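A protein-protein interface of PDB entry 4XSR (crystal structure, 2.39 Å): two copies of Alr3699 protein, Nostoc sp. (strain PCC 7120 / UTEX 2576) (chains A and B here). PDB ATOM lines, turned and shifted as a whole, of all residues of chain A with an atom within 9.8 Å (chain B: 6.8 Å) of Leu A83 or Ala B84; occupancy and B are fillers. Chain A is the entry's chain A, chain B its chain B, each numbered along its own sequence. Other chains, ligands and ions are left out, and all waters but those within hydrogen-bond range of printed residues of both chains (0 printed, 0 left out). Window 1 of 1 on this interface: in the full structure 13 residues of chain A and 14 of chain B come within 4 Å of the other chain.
Hydrophobic or aromatic side chains of chain B within 4 Å of the printed part of chain A: Ala B84, Leu B86 and Val B109.
Of the 18 printed residues of chain A, 7 touch a printed residue of chain B.
Hydrophobic or aromatic side chains of chain A within 4 Å of the printed part of chain B: Leu A80, Leu A83 and Ala A84.
Among the printed residues, 11 pairs touch across the chains.
Asn A62 touches Leu B83, and with the chains exchanged Leu A83 touches Asn B62.
Gln A82 touches Lys B106, and with the chains exchanged Lys A106 touches Gln B82.
Leu B83 touches its own counterpart, Leu A83.
Leu A83 touches Ala B84, and with the chains exchanged Ala A84 touches Leu B83.
14 positions are printed for both chains.
Printed residues of chain B within 4 Å of Leu A83: Asn B62 (3.2 Å), Leu B83 (3.97 Å), Ala B84 (3.6 Å) and Leu B86 (3.98 Å).
Ala B84 touches just one residue of chain A: Leu A83.
No residue of chain A comes within 4 Å of Pro B85.
No residue of chain A comes within 4 Å of Val B87.
Printed residues of chain B within 4 Å of Ala A84: Leu B83.
Printed residues of chain B within 4 Å of Leu A80: Val B109.
Printed residues of chain A within 4 Å of Val B109: Leu A80 (3.9 Å).
Gly A81 touches none of the printed residues of chain B.
Phe B41 touches none of the printed residues of chain A.
The nearest printed residue of chain B that does not touch Leu A83 is Val B109 (4.2 Å).
The nearest residue of chain A that does not touch Ala B84 is Ala A84 (4.7 Å).
The nearest printed residue of chain A that does not touch Asn B62 is Ala A84 (4.8 Å).
Among the printed residues, pairs that only touch across the chains: Leu A80 with Val B109 (3.9 Å), Gln A82 with Asn B62 (3.9 Å), Gln A82 with Lys B106 (3.9 Å), Leu A83 with Leu B83 (3.97 Å), Leu A83 with Ala B84 (3.6 Å), Leu A83 with Leu B86 (3.98 Å) and Ala A84 with Leu B83 (3.9 Å).
The backbone carbonyl oxygen (O) of Ser A79 lies within hydrogen-bond range of the side-chain amino group (NZ) of Lys B106, 3.2 Å away.
ND2 of Asn B62 sits at hydrogen-bond distance from O of Leu A83 (3.2 Å).
The side-chain amide oxygen of Gln B82 sits at hydrogen-bond distance from the side-chain amino group of Lys A106 (3.0 Å).
The side-chain amide nitrogen (ND2) of Asn A62 sits at hydrogen-bond distance from the backbone carbonyl oxygen (O) of Leu B83, 3.2 Å away.
The side-chain amide oxygen (OD1) of Asn A62 lies within hydrogen-bond range of the backbone NH (N) of Leu A86.
N of Leu B80 is in hydrogen-bond range of OE1 of Gln B82 (2.6 Å).
OD1 of Asn B62 lies within hydrogen-bond range of N of Leu B86 (3.2 Å).
The backbone carbonyl oxygen (O) of Thr B61 sits close to the backbone NH (N) of Leu B86 (3.4 Å).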
ATOM      1  N   ASN A  62      37.482  12.748 -13.178  1.00  0.00           N
ATOM      2  CA  ASN A  62      36.464  13.542 -12.512  1.00  0.00           C
ATOM      3  C   ASN A  62      36.838  13.814 -11.049  1.00  0.00           C
ATOM      4  O   ASN A  62      35.966  13.936 -10.200  1.00  0.00           O
ATOM      5  CB  ASN A  62      35.115  12.823 -12.623  1.00  0.00           C
ATOM      6  CG  ASN A  62      33.914  13.774 -12.636  1.00  0.00           C
ATOM      7  OD1 ASN A  62      33.902  14.861 -13.243  1.00  0.00           O
ATOM      8  ND2 ASN A  62      32.866  13.326 -11.996  1.00  0.00           N
ATOM      9  N   GLN A  63      38.134  13.901 -10.756  1.00  0.00           N
ATOM     10  CA  GLN A  63      38.591  14.467  -9.487  1.00  0.00           C
ATOM     11  C   GLN A  63      38.935  15.931  -9.739  1.00  0.00           C
ATOM     12  O   GLN A  63      39.084  16.305 -10.893  1.00  0.00           O
ATOM     13  CB  GLN A  63      39.785  13.698  -8.967  1.00  0.00           C
ATOM     14  CG  GLN A  63      39.445  12.261  -8.614  1.00  0.00           C
ATOM     15  CD  GLN A  63      40.682  11.449  -8.320  1.00  0.00           C
ATOM     16  OE1 GLN A  63      41.789  11.835  -8.699  1.00  0.00           O
ATOM     17  NE2 GLN A  63      40.508  10.322  -7.641  1.00  0.00           N
ATOM     18  N   PRO A  64      39.036  16.771  -8.673  1.00  0.00           N
ATOM     19  CA  PRO A  64      39.084  18.232  -8.891  1.00  0.00           C
ATOM     20  C   PRO A  64      40.464  18.867  -8.897  1.00  0.00           C
ATOM     21  O   PRO A  64      40.581  20.009  -9.356  1.00  0.00           O
ATOM     22  CB  PRO A  64      38.254  18.785  -7.722  1.00  0.00           C
ATOM     23  CG  PRO A  64      37.909  17.600  -6.848  1.00  0.00           C
ATOM     24  CD  PRO A  64      38.819  16.479  -7.248  1.00  0.00           C
ATOM     25  N   SER A  79      33.948  27.455 -10.403  1.00  0.00           N
ATOM     26  CA  SER A  79      32.605  27.944 -10.103  1.00  0.00           C
ATOM     27  C   SER A  79      31.598  26.823 -10.387  1.00  0.00           C
ATOM     28  O   SER A  79      31.434  25.911  -9.573  1.00  0.00           O
ATOM     29  CB  SER A  79      32.302  29.195 -10.937  1.00  0.00           C
ATOM     30  OG  SER A  79      32.227  28.871 -12.326  1.00  0.00           O
ATOM     31  N   LEU A  80      30.958  26.877 -11.557  1.00  0.00           N
ATOM     32  CA  LEU A  80      30.005  25.842 -11.991  1.00  0.00           C
ATOM     33  C   LEU A  80      30.731  24.493 -12.139  1.00  0.00           C
ATOM     34  O   LEU A  80      30.136  23.438 -11.903  1.00  0.00           O
ATOM     35  CB  LEU A  80      29.294  26.263 -13.297  1.00  0.00           C
ATOM     36  CG  LEU A  80      28.569  27.635 -13.275  1.00  0.00           C
ATOM     37  CD1 LEU A  80      28.486  28.266 -14.652  1.00  0.00           C
ATOM     38  CD2 LEU A  80      27.176  27.583 -12.656  1.00  0.00           C
ATOM     39  N   GLY A  81      32.029  24.546 -12.459  1.00  0.00           N
ATOM     40  CA  GLY A  81      32.892  23.365 -12.559  1.00  0.00           C
ATOM     41  C   GLY A  81      32.936  22.379 -11.404  1.00  0.00           C
ATOM     42  O   GLY A  81      33.369  21.257 -11.591  1.00  0.00           O
ATOM     43  N   GLN A  82      32.495  22.771 -10.209  1.00  0.00           N
ATOM     44  CA  GLN A  82      32.480  21.858  -9.038  1.00  0.00           C
ATOM     45  C   GLN A  82      31.527  20.667  -9.208  1.00  0.00           C
ATOM     46  O   GLN A  82      31.737  19.606  -8.625  1.00  0.00           O
ATOM     47  CB  GLN A  82      32.080  22.615  -7.759  1.00  0.00           C
ATOM     48  CG  GLN A  82      33.031  23.731  -7.316  1.00  0.00           C
ATOM     49  CD  GLN A  82      34.152  23.267  -6.380  1.00  0.00           C
ATOM     50  OE1 GLN A  82      33.912  22.626  -5.350  1.00  0.00           O
ATOM     51  NE2 GLN A  82      35.385  23.618  -6.726  1.00  0.00           N
ATOM     52  N   LEU A  83      30.466  20.864  -9.984  1.00  0.00           N
ATOM     53  CA  LEU A  83      29.465  19.809 -10.238  1.00  0.00           C
ATOM     54  C   LEU A  83      30.019  18.680 -11.124  1.00  0.00           C
ATOM     55  O   LEU A  83      29.589  17.523 -11.006  1.00  0.00           O
ATOM     56  CB  LEU A  83      28.221  20.404 -10.921  1.00  0.00           C
ATOM     57  CG  LEU A  83      27.523  21.608 -10.271  1.00  0.00           C
ATOM     58  CD1 LEU A  83      26.642  22.359 -11.268  1.00  0.00           C
ATOM     59  CD2 LEU A  83      26.726  21.155  -9.051  1.00  0.00           C
ATOM     60  N   ALA A  84      30.966  19.039 -12.001  1.00  0.00           N
ATOM     61  CA  ALA A  84      31.521  18.123 -12.995  1.00  0.00           C
ATOM     62  C   ALA A  84      32.954  18.510 -13.409  1.00  0.00           C
ATOM     63  O   ALA A  84      33.183  19.134 -14.447  1.00  0.00           O
ATOM     64  CB  ALA A  84      30.602  18.090 -14.200  1.00  0.00           C
ATOM     65  N   PRO A  85      33.939  18.141 -12.593  1.00  0.00           N
ATOM     66  CA  PRO A  85      35.282  18.657 -12.901  1.00  0.00           C
ATOM     67  C   PRO A  85      35.801  18.212 -14.289  1.00  0.00           C
ATOM     68  O   PRO A  85      36.319  19.049 -15.080  1.00  0.00           O
ATOM     69  CB  PRO A  85      36.155  18.143 -11.745  1.00  0.00           C
ATOM     70  CG  PRO A  85      35.240  17.458 -10.770  1.00  0.00           C
ATOM     71  CD  PRO A  85      33.828  17.488 -11.272  1.00  0.00           C
ATOM     72  N   LEU A  86      35.607  16.931 -14.611  1.00  0.00           N
ATOM     73  CA  LEU A  86      35.955  16.403 -15.950  1.00  0.00           C
ATOM     74  C   LEU A  86      35.474  17.331 -17.039  1.00  0.00           C
ATOM     75  O   LEU A  86      36.224  17.676 -17.966  1.00  0.00           O
ATOM     76  CB  LEU A  86      35.360  15.018 -16.151  1.00  0.00           C
ATOM     77  CG  LEU A  86      35.788  14.286 -17.423  1.00  0.00           C
ATOM     78  CD1 LEU A  86      35.897  12.786 -17.145  1.00  0.00           C
ATOM     79  CD2 LEU A  86      34.840  14.584 -18.581  1.00  0.00           C
ATOM     80  N   VAL A  87      34.238  17.791 -16.901  1.00  0.00           N
ATOM     81  CA  VAL A  87      33.688  18.726 -17.879  1.00  0.00           C
ATOM     82  C   VAL A  87      34.453  20.020 -17.908  1.00  0.00           C
ATOM     83  O   VAL A  87      34.635  20.622 -18.973  1.00  0.00           O
ATOM     84  CB  VAL A  87      32.226  19.053 -17.596  1.00  0.00           C
ATOM     85  CG1 VAL A  87      31.708  20.099 -18.589  1.00  0.00           C
ATOM     86  CG2 VAL A  87      31.382  17.786 -17.645  1.00  0.00           C
ATOM     87  N   ALA A  88      34.876  20.474 -16.733  1.00  0.00           N
ATOM     88  CA  ALA A  88      35.563  21.758 -16.639  1.00  0.00           C
ATOM     89  C   ALA A  88      36.942  21.629 -17.248  1.00  0.00           C
ATOM     90  O   ALA A  88      37.380  22.502 -18.003  1.00  0.00           O
ATOM     91  CB  ALA A  88      35.646  22.216 -15.188  1.00  0.00           C
ATOM     92  N   LYS A  89      37.622  20.526 -16.960  1.00  0.00           N
ATOM     93  CA  LYS A  89      38.906  20.277 -17.640  1.00  0.00           C
ATOM     94  C   LYS A  89      38.754  20.244 -19.167  1.00  0.00           C
ATOM     95  O   LYS A  89      39.570  20.848 -19.902  1.00  0.00           O
ATOM     96  CB  LYS A  89      39.540  19.000 -17.152  1.00  0.00           C
ATOM     97  CG  LYS A  89      39.820  19.000 -15.662  1.00  0.00           C
ATOM     98  CD  LYS A  89      40.192  17.610 -15.173  1.00  0.00           C
ATOM     99  CE  LYS A  89      40.133  17.489 -13.656  1.00  0.00           C
ATOM    100  NZ  LYS A  89      40.279  16.063 -13.237  1.00  0.00           N
ATOM    101  N   LYS A 106      28.497  10.042 -24.403  1.00  0.00           N
ATOM    102  CA  LYS A 106      28.919  10.869 -23.269  1.00  0.00           C
ATOM    103  C   LYS A 106      29.852  11.957 -23.730  1.00  0.00           C
ATOM    104  O   LYS A 106      29.837  13.090 -23.177  1.00  0.00           O
ATOM    105  CB  LYS A 106      29.563  10.065 -22.145  1.00  0.00           C
ATOM    106  CG  LYS A 106      28.586   9.172 -21.424  1.00  0.00           C
ATOM    107  CD  LYS A 106      29.180   8.564 -20.159  1.00  0.00           C
ATOM    108  CE  LYS A 106      28.449   7.263 -19.785  1.00  0.00           C
ATOM    109  NZ  LYS A 106      29.217   6.391 -18.844  1.00  0.00           N
ATOM    110  N   VAL A 109      27.768  14.824 -24.837  1.00  0.00           N
ATOM    111  CA  VAL A 109      27.291  15.646 -23.729  1.00  0.00           C
ATOM    112  C   VAL A 109      28.359  16.674 -23.389  1.00  0.00           C
ATOM    113  O   VAL A 109      28.127  17.871 -23.450  1.00  0.00           O
ATOM    114  CB  VAL A 109      27.015  14.826 -22.474  1.00  0.00           C
ATOM    115  CG1 VAL A 109      26.610  15.767 -21.331  1.00  0.00           C
ATOM    116  CG2 VAL A 109      25.960  13.760 -22.750  1.00  0.00           C
ATOM    117  N   VAL A 110      29.558  16.180 -23.123  1.00  0.00           N
ATOM    118  CA  VAL A 110      30.661  17.026 -22.720  1.00  0.00           C
ATOM    119  C   VAL A 110      31.121  17.911 -23.844  1.00  0.00           C
ATOM    120  O   VAL A 110      31.442  19.067 -23.627  1.00  0.00           O
ATOM    121  CB  VAL A 110      31.843  16.190 -22.242  1.00  0.00           C
ATOM    122  CG1 VAL A 110      33.010  17.088 -21.844  1.00  0.00           C
ATOM    123  CG2 VAL A 110      31.425  15.283 -21.099  1.00  0.00           C
ATOM    124  N   ILE A 113      28.641  20.879 -24.229  1.00  0.00           N
ATOM    125  CA  ILE A 113      28.941  21.866 -23.223  1.00  0.00           C
ATOM    126  C   ILE A 113      30.182  22.658 -23.624  1.00  0.00           C
ATOM    127  O   ILE A 113      30.110  23.864 -23.805  1.00  0.00           O
ATOM    128  CB  ILE A 113      29.074  21.205 -21.861  1.00  0.00           C
ATOM    129  CG1 ILE A 113      27.690  20.680 -21.425  1.00  0.00           C
ATOM    130  CG2 ILE A 113      29.643  22.188 -20.851  1.00  0.00           C
ATOM    131  CD1 ILE A 113      27.725  19.747 -20.229  1.00  0.00           C
ATOM    132  N   PHE B  41      22.663  21.541  -2.027  1.00  0.00           N
ATOM    133  CA  PHE B  41      23.817  20.862  -2.577  1.00  0.00           C
ATOM    134  C   PHE B  41      24.953  20.861  -1.577  1.00  0.00           C
ATOM    135  O   PHE B  41      26.101  20.635  -1.934  1.00  0.00           O
ATOM    136  CB  PHE B  41      24.281  21.531  -3.877  1.00  0.00           C
ATOM    137  CG  PHE B  41      23.211  21.639  -4.940  1.00  0.00           C
ATOM    138  CD1 PHE B  41      21.997  20.984  -4.821  1.00  0.00           C
ATOM    139  CD2 PHE B  41      23.445  22.391  -6.055  1.00  0.00           C
ATOM    140  CE1 PHE B  41      21.042  21.078  -5.801  1.00  0.00           C
ATOM    141  CE2 PHE B  41      22.495  22.504  -7.048  1.00  0.00           C
ATOM    142  CZ  PHE B  41      21.288  21.845  -6.920  1.00  0.00           C
ATOM    143  N   THR B  61      24.527  15.190  -2.552  1.00  0.00           N
ATOM    144  CA  THR B  61      25.994  15.249  -2.603  1.00  0.00           C
ATOM    145  C   THR B  61      26.478  14.770  -3.971  1.00  0.00           C
ATOM    146  O   THR B  61      25.669  14.305  -4.789  1.00  0.00           O
ATOM    147  CB  THR B  61      26.630  14.348  -1.533  1.00  0.00           C
ATOM    148  OG1 THR B  61      26.351  12.977  -1.852  1.00  0.00           O
ATOM    149  CG2 THR B  61      26.089  14.675  -0.132  1.00  0.00           C
ATOM    150  N   ASN B  62      27.787  14.868  -4.216  1.00  0.00           N
ATOM    151  CA  ASN B  62      28.349  14.364  -5.470  1.00  0.00           C
ATOM    152  C   ASN B  62      29.003  12.976  -5.317  1.00  0.00           C
ATOM    153  O   ASN B  62      29.765  12.566  -6.186  1.00  0.00           O
ATOM    154  CB  ASN B  62      29.335  15.385  -6.079  1.00  0.00           C
ATOM    155  CG  ASN B  62      29.135  15.600  -7.593  1.00  0.00           C
ATOM    156  OD1 ASN B  62      28.055  15.369  -8.158  1.00  0.00           O
ATOM    157  ND2 ASN B  62      30.183  16.084  -8.249  1.00  0.00           N
ATOM    158  N   LEU B  80      24.731   7.242 -17.630  1.00  0.00           N
ATOM    159  CA  LEU B  80      24.994   8.568 -18.207  1.00  0.00           C
ATOM    160  C   LEU B  80      25.158   9.701 -17.157  1.00  0.00           C
ATOM    161  O   LEU B  80      25.927  10.648 -17.364  1.00  0.00           O
ATOM    162  CB  LEU B  80      23.904   8.926 -19.238  1.00  0.00           C
ATOM    163  CG  LEU B  80      24.121  10.236 -20.039  1.00  0.00           C
ATOM    164  CD1 LEU B  80      23.889  10.087 -21.548  1.00  0.00           C
ATOM    165  CD2 LEU B  80      23.269  11.369 -19.474  1.00  0.00           C
ATOM    166  N   GLY B  81      24.443   9.604 -16.036  1.00  0.00           N
ATOM    167  CA  GLY B  81      24.617  10.539 -14.930  1.00  0.00           C
ATOM    168  C   GLY B  81      25.813  10.191 -14.061  1.00  0.00           C
ATOM    169  O   GLY B  81      25.850  10.526 -12.888  1.00  0.00           O
ATOM    170  N   GLN B  82      26.802   9.523 -14.635  1.00  0.00           N
ATOM    171  CA  GLN B  82      27.986   9.106 -13.895  1.00  0.00           C
ATOM    172  C   GLN B  82      28.964  10.273 -13.826  1.00  0.00           C
ATOM    173  O   GLN B  82      29.805  10.332 -12.947  1.00  0.00           O
ATOM    174  CB  GLN B  82      28.587   7.866 -14.564  1.00  0.00           C
ATOM    175  CG  GLN B  82      27.561   6.722 -14.641  1.00  0.00           C
ATOM    176  CD  GLN B  82      27.640   5.887 -15.911  1.00  0.00           C
ATOM    177  OE1 GLN B  82      26.932   6.150 -16.896  1.00  0.00           O
ATOM    178  NE2 GLN B  82      28.490   4.864 -15.892  1.00  0.00           N
ATOM    179  N   LEU B  83      28.797  11.223 -14.743  1.00  0.00           N
ATOM    180  CA  LEU B  83      29.554  12.480 -14.771  1.00  0.00           C
ATOM    181  C   LEU B  83      29.264  13.440 -13.603  1.00  0.00           C
ATOM    182  O   LEU B  83      30.080  14.320 -13.304  1.00  0.00           O
ATOM    183  CB  LEU B  83      29.199  13.234 -16.053  1.00  0.00           C
ATOM    184  CG  LEU B  83      29.425  12.550 -17.403  1.00  0.00           C
ATOM    185  CD1 LEU B  83      28.558  13.181 -18.489  1.00  0.00           C
ATOM    186  CD2 LEU B  83      30.904  12.606 -17.767  1.00  0.00           C
ATOM    187  N   ALA B  84      28.082  13.300 -12.994  1.00  0.00           N
ATOM    188  CA  ALA B  84      27.585  14.230 -11.975  1.00  0.00           C
ATOM    189  C   ALA B  84      26.495  13.548 -11.137  1.00  0.00           C
ATOM    190  O   ALA B  84      25.293  13.653 -11.443  1.00  0.00           O
ATOM    191  CB  ALA B  84      27.042  15.490 -12.640  1.00  0.00           C
ATOM    192  N   PRO B  85      26.910  12.808 -10.103  1.00  0.00           N
ATOM    193  CA  PRO B  85      25.994  12.032  -9.262  1.00  0.00           C
ATOM    194  C   PRO B  85      24.834  12.879  -8.716  1.00  0.00           C
ATOM    195  O   PRO B  85      23.654  12.518  -8.873  1.00  0.00           O
ATOM    196  CB  PRO B  85      26.899  11.538  -8.121  1.00  0.00           C
ATOM    197  CG  PRO B  85      28.289  11.552  -8.672  1.00  0.00           C
ATOM    198  CD  PRO B  85      28.328  12.515  -9.818  1.00  0.00           C
ATOM    199  N   LEU B  86      25.185  14.016  -8.112  1.00  0.00           N
ATOM    200  CA  LEU B  86      24.208  15.020  -7.636  1.00  0.00           C
ATOM    201  C   LEU B  86      23.108  15.309  -8.668  1.00  0.00           C
ATOM    202  O   LEU B  86      21.902  15.242  -8.353  1.00  0.00           O
ATOM    203  CB  LEU B  86      24.946  16.308  -7.260  1.00  0.00           C
ATOM    204  CG  LEU B  86      24.170  17.467  -6.621  1.00  0.00           C
ATOM    205  CD1 LEU B  86      24.866  17.926  -5.347  1.00  0.00           C
ATOM    206  CD2 LEU B  86      24.021  18.611  -7.611  1.00  0.00           C
ATOM    207  N   VAL B  87      23.503  15.571  -9.910  1.00  0.00           N
ATOM    208  CA  VAL B  87      22.490  15.881 -10.925  1.00  0.00           C
ATOM    209  C   VAL B  87      21.523  14.718 -11.144  1.00  0.00           C
ATOM    210  O   VAL B  87      20.320  14.922 -11.353  1.00  0.00           O
ATOM    211  CB  VAL B  87      23.105  16.279 -12.276  1.00  0.00           C
ATOM    212  CG1 VAL B  87      22.010  16.522 -13.314  1.00  0.00           C
ATOM    213  CG2 VAL B  87      24.008  17.496 -12.127  1.00  0.00           C
ATOM    214  N   ALA B  88      22.064  13.503 -11.095  1.00  0.00           N
ATOM    215  CA  ALA B  88      21.278  12.281 -11.302  1.00  0.00           C
ATOM    216  C   ALA B  88      20.271  12.089 -10.206  1.00  0.00           C
ATOM    217  O   ALA B  88      19.098  11.784 -10.473  1.00  0.00           O
ATOM    218  CB  ALA B  88      22.202  11.068 -11.352  1.00  0.00           C
ATOM    219  N   LYS B  89      20.746  12.259  -8.972  1.00  0.00           N
ATOM    220  CA  LYS B  89      19.890  12.165  -7.783  1.00  0.00           C
ATOM    221  C   LYS B  89      18.773  13.186  -7.848  1.00  0.00           C
ATOM    222  O   LYS B  89      17.618  12.867  -7.547  1.00  0.00           O
ATOM    223  CB  LYS B  89      20.691  12.384  -6.509  1.00  0.00           C
ATOM    224  CG  LYS B  89      21.928  11.497  -6.380  1.00  0.00           C
ATOM    225  CD  LYS B  89      22.605  11.624  -5.026  1.00  0.00           C
ATOM    226  CE  LYS B  89      23.988  10.986  -5.039  1.00  0.00           C
ATOM    227  NZ  LYS B  89      24.871  11.554  -3.978  1.00  0.00           N
ATOM    228  N   LYS B 106      23.792  27.708  -9.470  1.00  0.00           N
ATOM    229  CA  LYS B 106      24.078  26.271  -9.638  1.00  0.00           C
ATOM    230  C   LYS B 106      22.784  25.464  -9.609  1.00  0.00           C
ATOM    231  O   LYS B 106      22.632  24.505 -10.354  1.00  0.00           O
ATOM    232  CB  LYS B 106      25.045  25.744  -8.586  1.00  0.00           C
ATOM    233  CG  LYS B 106      26.454  26.271  -8.744  1.00  0.00           C
ATOM    234  CD  LYS B 106      27.440  25.641  -7.747  1.00  0.00           C
ATOM    235  CE  LYS B 106      28.772  26.410  -7.740  1.00  0.00           C
ATOM    236  NZ  LYS B 106      29.826  25.829  -6.855  1.00  0.00           N
ATOM    237  N   ALA B 107      21.840  25.888  -8.780  1.00  0.00           N
ATOM    238  CA  ALA B 107      20.563  25.238  -8.732  1.00  0.00           C
ATOM    239  C   ALA B 107      19.788  25.377 -10.012  1.00  0.00           C
ATOM    240  O   ALA B 107      18.927  24.556 -10.284  1.00  0.00           O
ATOM    241  CB  ALA B 107      19.742  25.767  -7.598  1.00  0.00           C
ATOM    242  N   VAL B 109      21.283  25.357 -13.086  1.00  0.00           N
ATOM    243  CA  VAL B 109      21.941  24.390 -13.947  1.00  0.00           C
ATOM    244  C   VAL B 109      21.372  22.997 -13.704  1.00  0.00           C
ATOM    245  O   VAL B 109      20.870  22.335 -14.610  1.00  0.00           O
ATOM    246  CB  VAL B 109      23.454  24.397 -13.699  1.00  0.00           C
ATOM    247  CG1 VAL B 109      24.128  23.313 -14.522  1.00  0.00           C
ATOM    248  CG2 VAL B 109      24.036  25.768 -14.033  1.00  0.00           C
ATOM    249  N   VAL B 110      21.380  22.591 -12.448  1.00  0.00           N
ATOM    250  CA  VAL B 110      20.836  21.289 -12.065  1.00  0.00           C
ATOM    251  C   VAL B 110      19.331  21.199 -12.323  1.00  0.00           C
ATOM    252  O   VAL B 110      18.852  20.200 -12.849  1.00  0.00           O
ATOM    253  CB  VAL B 110      21.158  20.995 -10.591  1.00  0.00           C
ATOM    254  CG1 VAL B 110      20.506  19.709 -10.128  1.00  0.00           C
ATOM    255  CG2 VAL B 110      22.661  20.989 -10.358  1.00  0.00           C
